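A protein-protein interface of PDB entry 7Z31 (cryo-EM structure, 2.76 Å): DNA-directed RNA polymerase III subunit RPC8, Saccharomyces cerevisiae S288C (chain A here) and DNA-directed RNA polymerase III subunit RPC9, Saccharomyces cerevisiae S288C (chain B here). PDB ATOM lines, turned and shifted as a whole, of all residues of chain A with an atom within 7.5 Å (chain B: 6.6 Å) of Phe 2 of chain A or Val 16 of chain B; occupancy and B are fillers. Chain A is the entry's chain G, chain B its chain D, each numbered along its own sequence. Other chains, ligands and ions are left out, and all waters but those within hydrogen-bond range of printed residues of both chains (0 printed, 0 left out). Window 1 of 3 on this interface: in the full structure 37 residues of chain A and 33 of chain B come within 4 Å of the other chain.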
ATOM      1  N   PHE A   2     -24.723   0.014  34.155  1.00  0.00           N
ATOM      2  CA  PHE A   2     -24.749  -0.151  32.706  1.00  0.00           C
ATOM      3  C   PHE A   2     -23.339  -0.279  32.141  1.00  0.00           C
ATOM      4  O   PHE A   2     -22.701   0.715  31.794  1.00  0.00           O
ATOM      5  CB  PHE A   2     -25.481   1.021  32.049  1.00  0.00           C
ATOM      6  CG  PHE A   2     -26.909   0.717  31.687  1.00  0.00           C
ATOM      7  CD1 PHE A   2     -27.801   0.278  32.646  1.00  0.00           C
ATOM      8  CD2 PHE A   2     -27.356   0.874  30.391  1.00  0.00           C
ATOM      9  CE1 PHE A   2     -29.115  -0.007  32.318  1.00  0.00           C
ATOM     10  CE2 PHE A   2     -28.670   0.595  30.054  1.00  0.00           C
ATOM     11  CZ  PHE A   2     -29.549   0.156  31.020  1.00  0.00           C
ATOM     12  N   ILE A   3     -22.856  -1.518  32.054  1.00  0.00           N
ATOM     13  CA  ILE A   3     -21.538  -1.815  31.517  1.00  0.00           C
ATOM     14  C   ILE A   3     -21.660  -2.958  30.517  1.00  0.00           C
ATOM     15  O   ILE A   3     -22.666  -3.666  30.466  1.00  0.00           O
ATOM     16  CB  ILE A   3     -20.522  -2.176  32.617  1.00  0.00           C
ATOM     17  CG1 ILE A   3     -21.044  -3.348  33.448  1.00  0.00           C
ATOM     18  CG2 ILE A   3     -20.243  -0.972  33.493  1.00  0.00           C
ATOM     19  CD1 ILE A   3     -19.977  -4.067  34.242  1.00  0.00           C
ATOM     20  N   LEU A   4     -20.612  -3.129  29.718  1.00  0.00           N
ATOM     21  CA  LEU A   4     -20.581  -4.150  28.685  1.00  0.00           C
ATOM     22  C   LEU A   4     -20.122  -5.488  29.261  1.00  0.00           C
ATOM     23  O   LEU A   4     -19.884  -5.634  30.463  1.00  0.00           O
ATOM     24  CB  LEU A   4     -19.673  -3.715  27.538  1.00  0.00           C
ATOM     25  CG  LEU A   4     -20.366  -2.958  26.410  1.00  0.00           C
ATOM     26  CD1 LEU A   4     -19.368  -2.502  25.361  1.00  0.00           C
ATOM     27  CD2 LEU A   4     -21.414  -3.845  25.797  1.00  0.00           C
ATOM     28  N   LEU A  44     -28.451  -8.444  33.783  1.00  0.00           N
ATOM     29  CA  LEU A  44     -29.545  -8.324  32.833  1.00  0.00           C
ATOM     30  C   LEU A  44     -28.998  -7.803  31.514  1.00  0.00           C
ATOM     31  O   LEU A  44     -28.412  -6.721  31.476  1.00  0.00           O
ATOM     32  CB  LEU A  44     -30.624  -7.376  33.365  1.00  0.00           C
ATOM     33  CG  LEU A  44     -31.907  -7.095  32.573  1.00  0.00           C
ATOM     34  CD1 LEU A  44     -32.964  -6.585  33.527  1.00  0.00           C
ATOM     35  CD2 LEU A  44     -31.708  -6.090  31.459  1.00  0.00           C
ATOM     36  N   ILE A  46     -29.386  -5.888  28.328  1.00  0.00           N
ATOM     37  CA  ILE A  46     -30.252  -4.932  27.646  1.00  0.00           C
ATOM     38  C   ILE A  46     -30.387  -5.305  26.176  1.00  0.00           C
ATOM     39  O   ILE A  46     -31.481  -5.613  25.691  1.00  0.00           O
ATOM     40  CB  ILE A  46     -29.718  -3.499  27.812  1.00  0.00           C
ATOM     41  CG1 ILE A  46     -29.781  -3.066  29.276  1.00  0.00           C
ATOM     42  CG2 ILE A  46     -30.521  -2.543  26.958  1.00  0.00           C
ATOM     43  CD1 ILE A  46     -31.186  -2.952  29.814  1.00  0.00           C
ATOM     44  N   THR A  47     -29.275  -5.288  25.451  1.00  0.00           N
ATOM     45  CA  THR A  47     -29.234  -5.689  24.052  1.00  0.00           C
ATOM     46  C   THR A  47     -27.781  -5.978  23.691  1.00  0.00           C
ATOM     47  O   THR A  47     -26.912  -6.052  24.565  1.00  0.00           O
ATOM     48  CB  THR A  47     -29.861  -4.622  23.143  1.00  0.00           C
ATOM     49  OG1 THR A  47     -29.521  -4.895  21.778  1.00  0.00           O
ATOM     50  CG2 THR A  47     -29.375  -3.233  23.510  1.00  0.00           C
ATOM     51  N   TYR A  49     -24.328  -4.869  21.860  1.00  0.00           N
ATOM     52  CA  TYR A  49     -23.660  -3.633  21.477  1.00  0.00           C
ATOM     53  C   TYR A  49     -22.984  -3.766  20.118  1.00  0.00           C
ATOM     54  O   TYR A  49     -23.286  -3.012  19.188  1.00  0.00           O
ATOM     55  CB  TYR A  49     -22.643  -3.241  22.547  1.00  0.00           C
ATOM     56  CG  TYR A  49     -22.176  -1.805  22.463  1.00  0.00           C
ATOM     57  CD1 TYR A  49     -23.038  -0.760  22.764  1.00  0.00           C
ATOM     58  CD2 TYR A  49     -20.873  -1.498  22.102  1.00  0.00           C
ATOM     59  CE1 TYR A  49     -22.619   0.548  22.703  1.00  0.00           C
ATOM     60  CE2 TYR A  49     -20.441  -0.188  22.038  1.00  0.00           C
ATOM     61  CZ  TYR A  49     -21.318   0.831  22.340  1.00  0.00           C
ATOM     62  OH  TYR A  49     -20.900   2.137  22.275  1.00  0.00           O
ATOM     63  N   VAL A  75     -24.671  -5.069  26.312  1.00  0.00           N
ATOM     64  CA  VAL A  75     -24.863  -4.082  27.370  1.00  0.00           C
ATOM     65  C   VAL A  75     -25.717  -4.693  28.472  1.00  0.00           C
ATOM     66  O   VAL A  75     -26.830  -5.168  28.223  1.00  0.00           O
ATOM     67  CB  VAL A  75     -25.498  -2.796  26.816  1.00  0.00           C
ATOM     68  CG1 VAL A  75     -24.468  -1.981  26.050  1.00  0.00           C
ATOM     69  CG2 VAL A  75     -26.666  -3.117  25.917  1.00  0.00           C
ATOM     70  N   VAL A  76     -25.190  -4.692  29.695  1.00  0.00           N
ATOM     71  CA  VAL A  76     -25.873  -5.264  30.847  1.00  0.00           C
ATOM     72  C   VAL A  76     -25.859  -4.257  31.989  1.00  0.00           C
ATOM     73  O   VAL A  76     -24.915  -3.473  32.132  1.00  0.00           O
ATOM     74  CB  VAL A  76     -25.237  -6.599  31.296  1.00  0.00           C
ATOM     75  CG1 VAL A  76     -25.391  -7.654  30.215  1.00  0.00           C
ATOM     76  CG2 VAL A  76     -23.772  -6.408  31.646  1.00  0.00           C
ATOM     77  N   PHE A  77     -26.914  -4.277  32.798  1.00  0.00           N
ATOM     78  CA  PHE A  77     -27.005  -3.420  33.973  1.00  0.00           C
ATOM     79  C   PHE A  77     -26.232  -4.063  35.116  1.00  0.00           C
ATOM     80  O   PHE A  77     -26.565  -5.171  35.548  1.00  0.00           O
ATOM     81  CB  PHE A  77     -28.467  -3.211  34.360  1.00  0.00           C
ATOM     82  CG  PHE A  77     -28.692  -2.056  35.300  1.00  0.00           C
ATOM     83  CD1 PHE A  77     -27.651  -1.209  35.653  1.00  0.00           C
ATOM     84  CD2 PHE A  77     -29.948  -1.820  35.833  1.00  0.00           C
ATOM     85  CE1 PHE A  77     -27.860  -0.145  36.512  1.00  0.00           C
ATOM     86  CE2 PHE A  77     -30.161  -0.760  36.697  1.00  0.00           C
ATOM     87  CZ  PHE A  77     -29.116   0.076  37.036  1.00  0.00           C
ATOM     88  N   LYS A  78     -25.210  -3.369  35.618  1.00  0.00           N
ATOM     89  CA  LYS A  78     -24.354  -3.900  36.678  1.00  0.00           C
ATOM     90  C   LYS A  78     -23.941  -2.819  37.666  1.00  0.00           C
ATOM     91  O   LYS A  78     -22.854  -2.239  37.553  1.00  0.00           O
ATOM     92  CB  LYS A  78     -23.108  -4.572  36.099  1.00  0.00           C
ATOM     93  CG  LYS A  78     -23.344  -5.956  35.558  1.00  0.00           C
ATOM     94  CD  LYS A  78     -24.092  -6.796  36.568  1.00  0.00           C
ATOM     95  CE  LYS A  78     -23.246  -7.126  37.786  1.00  0.00           C
ATOM     96  NZ  LYS A  78     -23.997  -7.973  38.750  1.00  0.00           N
ATOM     97  N   PRO A  79     -24.786  -2.516  38.649  1.00  0.00           N
ATOM     98  CA  PRO A  79     -24.304  -1.786  39.828  1.00  0.00           C
ATOM     99  C   PRO A  79     -23.362  -2.656  40.647  1.00  0.00           C
ATOM    100  O   PRO A  79     -23.507  -3.880  40.696  1.00  0.00           O
ATOM    101  CB  PRO A  79     -25.589  -1.472  40.601  1.00  0.00           C
ATOM    102  CG  PRO A  79     -26.693  -1.605  39.594  1.00  0.00           C
ATOM    103  CD  PRO A  79     -26.250  -2.676  38.656  1.00  0.00           C
ATOM    104  N   GLU A  83     -23.542   2.730  43.177  1.00  0.00           N
ATOM    105  CA  GLU A  83     -24.174   3.324  42.010  1.00  0.00           C
ATOM    106  C   GLU A  83     -25.512   3.948  42.387  1.00  0.00           C
ATOM    107  O   GLU A  83     -26.237   3.428  43.241  1.00  0.00           O
ATOM    108  CB  GLU A  83     -24.365   2.286  40.903  1.00  0.00           C
ATOM    109  CG  GLU A  83     -23.129   1.440  40.618  1.00  0.00           C
ATOM    110  CD  GLU A  83     -21.996   2.216  39.967  1.00  0.00           C
ATOM    111  OE1 GLU A  83     -21.288   2.960  40.680  1.00  0.00           O
ATOM    112  OE2 GLU A  83     -21.806   2.072  38.739  1.00  0.00           O
ATOM    113  N   ILE A 104     -38.110  -2.083  33.670  1.00  0.00           N
ATOM    114  CA  ILE A 104     -36.865  -2.787  33.373  1.00  0.00           C
ATOM    115  C   ILE A 104     -36.739  -4.042  34.231  1.00  0.00           C
ATOM    116  O   ILE A 104     -36.713  -5.165  33.714  1.00  0.00           O
ATOM    117  CB  ILE A 104     -35.662  -1.843  33.555  1.00  0.00           C
ATOM    118  CG1 ILE A 104     -35.669  -0.771  32.459  1.00  0.00           C
ATOM    119  CG2 ILE A 104     -34.360  -2.613  33.522  1.00  0.00           C
ATOM    120  CD1 ILE A 104     -34.428   0.095  32.431  1.00  0.00           C
ATOM    121  N   PHE A 105     -36.667  -3.870  35.549  1.00  0.00           N
ATOM    122  CA  PHE A 105     -36.854  -4.973  36.485  1.00  0.00           C
ATOM    123  C   PHE A 105     -37.201  -4.381  37.843  1.00  0.00           C
ATOM    124  O   PHE A 105     -36.565  -3.415  38.277  1.00  0.00           O
ATOM    125  CB  PHE A 105     -35.616  -5.887  36.568  1.00  0.00           C
ATOM    126  CG  PHE A 105     -34.402  -5.234  37.154  1.00  0.00           C
ATOM    127  CD1 PHE A 105     -33.507  -4.556  36.346  1.00  0.00           C
ATOM    128  CD2 PHE A 105     -34.142  -5.318  38.509  1.00  0.00           C
ATOM    129  CE1 PHE A 105     -32.384  -3.962  36.879  1.00  0.00           C
ATOM    130  CE2 PHE A 105     -33.029  -4.726  39.045  1.00  0.00           C
ATOM    131  CZ  PHE A 105     -32.143  -4.045  38.229  1.00  0.00           C
ATOM    132  N   ALA B   9     -15.084  -2.744  29.422  1.00  0.00           N
ATOM    133  CA  ALA B   9     -14.873  -1.309  29.561  1.00  0.00           C
ATOM    134  C   ALA B   9     -16.146  -0.596  30.003  1.00  0.00           C
ATOM    135  O   ALA B   9     -17.218  -0.814  29.439  1.00  0.00           O
ATOM    136  CB  ALA B   9     -14.381  -0.731  28.233  1.00  0.00           C
ATOM    137  N   PHE B  10     -16.009   0.270  31.010  1.00  0.00           N
ATOM    138  CA  PHE B  10     -17.153   0.965  31.586  1.00  0.00           C
ATOM    139  C   PHE B  10     -17.867   1.804  30.534  1.00  0.00           C
ATOM    140  O   PHE B  10     -17.266   2.278  29.566  1.00  0.00           O
ATOM    141  CB  PHE B  10     -16.711   1.877  32.735  1.00  0.00           C
ATOM    142  CG  PHE B  10     -16.458   1.158  34.029  1.00  0.00           C
ATOM    143  CD1 PHE B  10     -17.510   0.643  34.765  1.00  0.00           C
ATOM    144  CD2 PHE B  10     -15.174   1.025  34.524  1.00  0.00           C
ATOM    145  CE1 PHE B  10     -17.286  -0.014  35.954  1.00  0.00           C
ATOM    146  CE2 PHE B  10     -14.940   0.371  35.719  1.00  0.00           C
ATOM    147  CZ  PHE B  10     -15.998  -0.148  36.434  1.00  0.00           C
ATOM    148  N   LEU B  11     -19.167   1.993  30.738  1.00  0.00           N
ATOM    149  CA  LEU B  11     -19.993   2.825  29.874  1.00  0.00           C
ATOM    150  C   LEU B  11     -20.554   3.983  30.683  1.00  0.00           C
ATOM    151  O   LEU B  11     -21.176   3.769  31.729  1.00  0.00           O
ATOM    152  CB  LEU B  11     -21.134   2.021  29.250  1.00  0.00           C
ATOM    153  CG  LEU B  11     -20.812   1.136  28.046  1.00  0.00           C
ATOM    154  CD1 LEU B  11     -19.998   1.903  27.016  1.00  0.00           C
ATOM    155  CD2 LEU B  11     -20.091  -0.116  28.485  1.00  0.00           C
ATOM    156  N   SER B  12     -20.334   5.200  30.200  1.00  0.00           N
ATOM    157  CA  SER B  12     -21.022   6.361  30.740  1.00  0.00           C
ATOM    158  C   SER B  12     -22.443   6.414  30.193  1.00  0.00           C
ATOM    159  O   SER B  12     -22.731   5.898  29.110  1.00  0.00           O
ATOM    160  CB  SER B  12     -20.275   7.648  30.386  1.00  0.00           C
ATOM    161  OG  SER B  12     -19.039   7.737  31.072  1.00  0.00           O
ATOM    162  N   ASP B  13     -23.336   7.049  30.949  1.00  0.00           N
ATOM    163  CA  ASP B  13     -24.720   7.147  30.503  1.00  0.00           C
ATOM    164  C   ASP B  13     -24.912   8.293  29.518  1.00  0.00           C
ATOM    165  O   ASP B  13     -25.782   9.147  29.711  1.00  0.00           O
ATOM    166  CB  ASP B  13     -25.661   7.315  31.695  1.00  0.00           C
ATOM    167  CG  ASP B  13     -25.661   6.111  32.612  1.00  0.00           C
ATOM    168  OD1 ASP B  13     -25.330   5.007  32.140  1.00  0.00           O
ATOM    169  OD2 ASP B  13     -25.995   6.266  33.806  1.00  0.00           O
ATOM    170  N   TYR B  14     -24.088   8.331  28.473  1.00  0.00           N
ATOM    171  CA  TYR B  14     -24.385   9.123  27.286  1.00  0.00           C
ATOM    172  C   TYR B  14     -24.169   8.264  26.049  1.00  0.00           C
ATOM    173  O   TYR B  14     -24.928   8.353  25.077  1.00  0.00           O
ATOM    174  CB  TYR B  14     -23.523  10.382  27.219  1.00  0.00           C
ATOM    175  CG  TYR B  14     -23.561  11.071  25.873  1.00  0.00           C
ATOM    176  CD1 TYR B  14     -24.747  11.586  25.367  1.00  0.00           C
ATOM    177  CD2 TYR B  14     -22.409  11.212  25.110  1.00  0.00           C
ATOM    178  CE1 TYR B  14     -24.787  12.218  24.135  1.00  0.00           C
ATOM    179  CE2 TYR B  14     -22.439  11.844  23.882  1.00  0.00           C
ATOM    180  CZ  TYR B  14     -23.630  12.345  23.399  1.00  0.00           C
ATOM    181  OH  TYR B  14     -23.657  12.974  22.175  1.00  0.00           O
ATOM    182  N   GLU B  15     -23.131   7.425  26.081  1.00  0.00           N
ATOM    183  CA  GLU B  15     -22.897   6.507  24.975  1.00  0.00           C
ATOM    184  C   GLU B  15     -24.033   5.501  24.857  1.00  0.00           C
ATOM    185  O   GLU B  15     -24.468   5.172  23.748  1.00  0.00           O
ATOM    186  CB  GLU B  15     -21.553   5.799  25.149  1.00  0.00           C
ATOM    187  CG  GLU B  15     -20.365   6.748  25.167  1.00  0.00           C
ATOM    188  CD  GLU B  15     -19.040   6.037  24.960  1.00  0.00           C
ATOM    189  OE1 GLU B  15     -19.040   4.792  24.858  1.00  0.00           O
ATOM    190  OE2 GLU B  15     -17.998   6.726  24.897  1.00  0.00           O
ATOM    191  N   VAL B  16     -24.543   5.018  25.992  1.00  0.00           N
ATOM    192  CA  VAL B  16     -25.670   4.091  25.953  1.00  0.00           C
ATOM    193  C   VAL B  16     -26.893   4.764  25.343  1.00  0.00           C
ATOM    194  O   VAL B  16     -27.611   4.163  24.534  1.00  0.00           O
ATOM    195  CB  VAL B  16     -25.960   3.532  27.359  1.00  0.00           C
ATOM    196  CG1 VAL B  16     -26.204   4.654  28.355  1.00  0.00           C
ATOM    197  CG2 VAL B  16     -27.140   2.574  27.314  1.00  0.00           C
ATOM    198  N   LEU B  17     -27.147   6.023  25.708  1.00  0.00           N
ATOM    199  CA  LEU B  17     -28.318   6.708  25.175  1.00  0.00           C
ATOM    200  C   LEU B  17     -28.164   6.996  23.690  1.00  0.00           C
ATOM    201  O   LEU B  17     -29.122   6.844  22.925  1.00  0.00           O
ATOM    202  CB  LEU B  17     -28.586   8.002  25.938  1.00  0.00           C
ATOM    203  CG  LEU B  17     -29.819   8.744  25.416  1.00  0.00           C
ATOM    204  CD1 LEU B  17     -31.015   7.804  25.359  1.00  0.00           C
ATOM    205  CD2 LEU B  17     -30.140   9.951  26.270  1.00  0.00           C
ATOM    206  N   LYS B  18     -26.977   7.428  23.257  1.00  0.00           N
ATOM    207  CA  LYS B  18     -26.798   7.657  21.830  1.00  0.00           C
ATOM    208  C   LYS B  18     -26.908   6.353  21.053  1.00  0.00           C
ATOM    209  O   LYS B  18     -27.450   6.343  19.944  1.00  0.00           O
ATOM    210  CB  LYS B  18     -25.466   8.360  21.547  1.00  0.00           C
ATOM    211  CG  LYS B  18     -24.210   7.534  21.767  1.00  0.00           C
ATOM    212  CD  LYS B  18     -22.972   8.274  21.269  1.00  0.00           C
ATOM    213  CE  LYS B  18     -21.693   7.595  21.735  1.00  0.00           C
ATOM    214  NZ  LYS B  18     -20.477   8.203  21.139  1.00  0.00           N
ATOM    215  N   PHE B  19     -26.445   5.244  21.634  1.00  0.00           N
ATOM    216  CA  PHE B  19     -26.590   3.949  20.980  1.00  0.00           C
ATOM    217  C   PHE B  19     -28.057   3.551  20.861  1.00  0.00           C
ATOM    218  O   PHE B  19     -28.491   3.060  19.815  1.00  0.00           O
ATOM    219  CB  PHE B  19     -25.797   2.888  21.748  1.00  0.00           C
ATOM    220  CG  PHE B  19     -26.028   1.492  21.260  1.00  0.00           C
ATOM    221  CD1 PHE B  19     -25.455   1.053  20.079  1.00  0.00           C
ATOM    222  CD2 PHE B  19     -26.826   0.617  21.981  1.00  0.00           C
ATOM    223  CE1 PHE B  19     -25.672  -0.233  19.628  1.00  0.00           C
ATOM    224  CE2 PHE B  19     -27.045  -0.668  21.536  1.00  0.00           C
ATOM    225  CZ  PHE B  19     -26.466  -1.094  20.356  1.00  0.00           C
ATOM    226  N   LEU B  20     -28.840   3.750  21.922  1.00  0.00           N
ATOM    227  CA  LEU B  20     -30.251   3.378  21.854  1.00  0.00           C
ATOM    228  C   LEU B  20     -31.019   4.289  20.903  1.00  0.00           C
ATOM    229  O   LEU B  20     -31.945   3.843  20.211  1.00  0.00           O
ATOM    230  CB  LEU B  20     -30.872   3.395  23.248  1.00  0.00           C
ATOM    231  CG  LEU B  20     -30.893   2.035  23.951  1.00  0.00           C
ATOM    232  CD1 LEU B  20     -29.613   1.786  24.720  1.00  0.00           C
ATOM    233  CD2 LEU B  20     -32.095   1.928  24.854  1.00  0.00           C
ATOM    234  N   THR B  21     -30.640   5.569  20.854  1.00  0.00           N
ATOM    235  CA  THR B  21     -31.209   6.488  19.878  1.00  0.00           C
ATOM    236  C   THR B  21     -30.893   6.034  18.461  1.00  0.00           C
ATOM    237  O   THR B  21     -31.762   6.054  17.584  1.00  0.00           O
ATOM    238  CB  THR B  21     -30.669   7.899  20.115  1.00  0.00           C
ATOM    239  OG1 THR B  21     -30.351   8.062  21.504  1.00  0.00           O
ATOM    240  CG2 THR B  21     -31.702   8.933  19.715  1.00  0.00           C
ATOM    241  N   VAL B  62     -35.198   1.846  28.588  1.00  0.00           N
ATOM    242  CA  VAL B  62     -33.911   2.460  28.907  1.00  0.00           C
ATOM    243  C   VAL B  62     -33.863   3.898  28.399  1.00  0.00           C
ATOM    244  O   VAL B  62     -33.447   4.818  29.117  1.00  0.00           O
ATOM    245  CB  VAL B  62     -32.754   1.621  28.338  1.00  0.00           C
ATOM    246  CG1 VAL B  62     -31.433   2.328  28.565  1.00  0.00           C
ATOM    247  CG2 VAL B  62     -32.733   0.250  28.975  1.00  0.00           C
ATOM    248  N   LEU B  66     -33.533   7.429  30.545  1.00  0.00           N
ATOM    249  CA  LEU B  66     -32.495   8.427  30.318  1.00  0.00           C
ATOM    250  C   LEU B  66     -33.052   9.730  29.757  1.00  0.00           C
ATOM    251  O   LEU B  66     -32.420  10.779  29.926  1.00  0.00           O
ATOM    252  CB  LEU B  66     -31.404   7.863  29.399  1.00  0.00           C
ATOM    253  CG  LEU B  66     -30.306   7.082  30.137  1.00  0.00           C
ATOM    254  CD1 LEU B  66     -30.797   5.711  30.578  1.00  0.00           C
ATOM    255  CD2 LEU B  66     -29.034   6.962  29.312  1.00  0.00           C
ATOM    256  N   LEU B 121     -18.110   7.983  36.419  1.00  0.00           N
ATOM    257  CA  LEU B 121     -19.382   7.648  35.787  1.00  0.00           C
ATOM    258  C   LEU B 121     -20.579   8.016  36.652  1.00  0.00           C
ATOM    259  O   LEU B 121     -21.669   8.251  36.117  1.00  0.00           O
ATOM    260  CB  LEU B 121     -19.429   6.156  35.432  1.00  0.00           C
ATOM    261  CG  LEU B 121     -19.943   5.168  36.479  1.00  0.00           C
ATOM    262  CD1 LEU B 121     -20.660   4.006  35.809  1.00  0.00           C
ATOM    263  CD2 LEU B 121     -18.794   4.660  37.339  1.00  0.00           C
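O of Leu 11 of chain B sits close to O of Phe 2 of chain A (3.4 Å).
N of Val 76 of chain A is in hydrogen-bond range of O of Ile 3 of chain A, 2.8 Å away. The backbone NH (N) of Ile 46 of chain A sits at hydrogen-bond distance from the backbone carbonyl oxygen (O) of Val 75 of chain A, 2.7 Å away. N of Val 75 of chain A lies within hydrogen-bond range of O of Thr 47 of chain A.
Asp 13 of chain B touches Phe 2 of chain A (OD1 to CB, 3.99 Å). Phe 2 of chain A touches Val 62 of chain B. Phe 10 of chain B touches Ile 3 of chain A. Ile 3 of chain A touches Leu 11 of chain B. CD2 of Leu 11 of chain B touches N of Leu 4 of chain A, at 3.3 Å. Ile 46 of chain A touches Val 62 of chain B (CD1 to CG2, 3.7 Å). CE2 of Phe 19 of chain B touches CG2 of Thr 47 of chain A, 3.99 Å away. Tyr 49 of chain A touches Phe 19 of chain B (O to CE1, 3.7 Å). Glu 83 of chain A touches Leu 121 of chain B. Ile 104 of chain A touches Val 62 of chain B.
Of chain A, only Phe 2 comes within 4 Å of Val 16 of chain B. Of the printed residues of chain B, Ile 46 of chain A touches Val 62. Printed residues of chain B within 4 Å of Glu 83 of chain A: Leu 121 (3.7 Å). Of the printed residues of chain B, Tyr 49 of chain A touches Phe 19 (3.7 Å). Printed residues of chain B within 4 Å of Ile 3 of chain A: Phe 10 (3.4 Å) and Leu 11 (3.8 Å). Val 76 of chain A touches none of the printed residues of chain B. The nearest printed residue of chain B that does not touch Phe 2 of chain A is Phe 10 of chain B (5.1 Å). The nearest residue of chain A that does not touch Val 16 of chain B is Val 75 of chain A (5.4 Å). The nearest printed residue of chain A that does not touch Phe 19 of chain B is Val 75 of chain A (5.0 Å).
Printed residues of chain A that touch a printed residue of chain B: Phe 2, Ile 3, Leu 4, Ile 46, Thr 47, Tyr 49, Glu 83 and Ile 104. Hydrophobic or aromatic side chains of chain A within 4 Å of the printed part of chain B: Phe 2, Ile 3, Leu 4, Ile 46, Tyr 49 and Ile 104. Of the 16 printed residues of chain B, 7 touch a printed residue of chain A.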
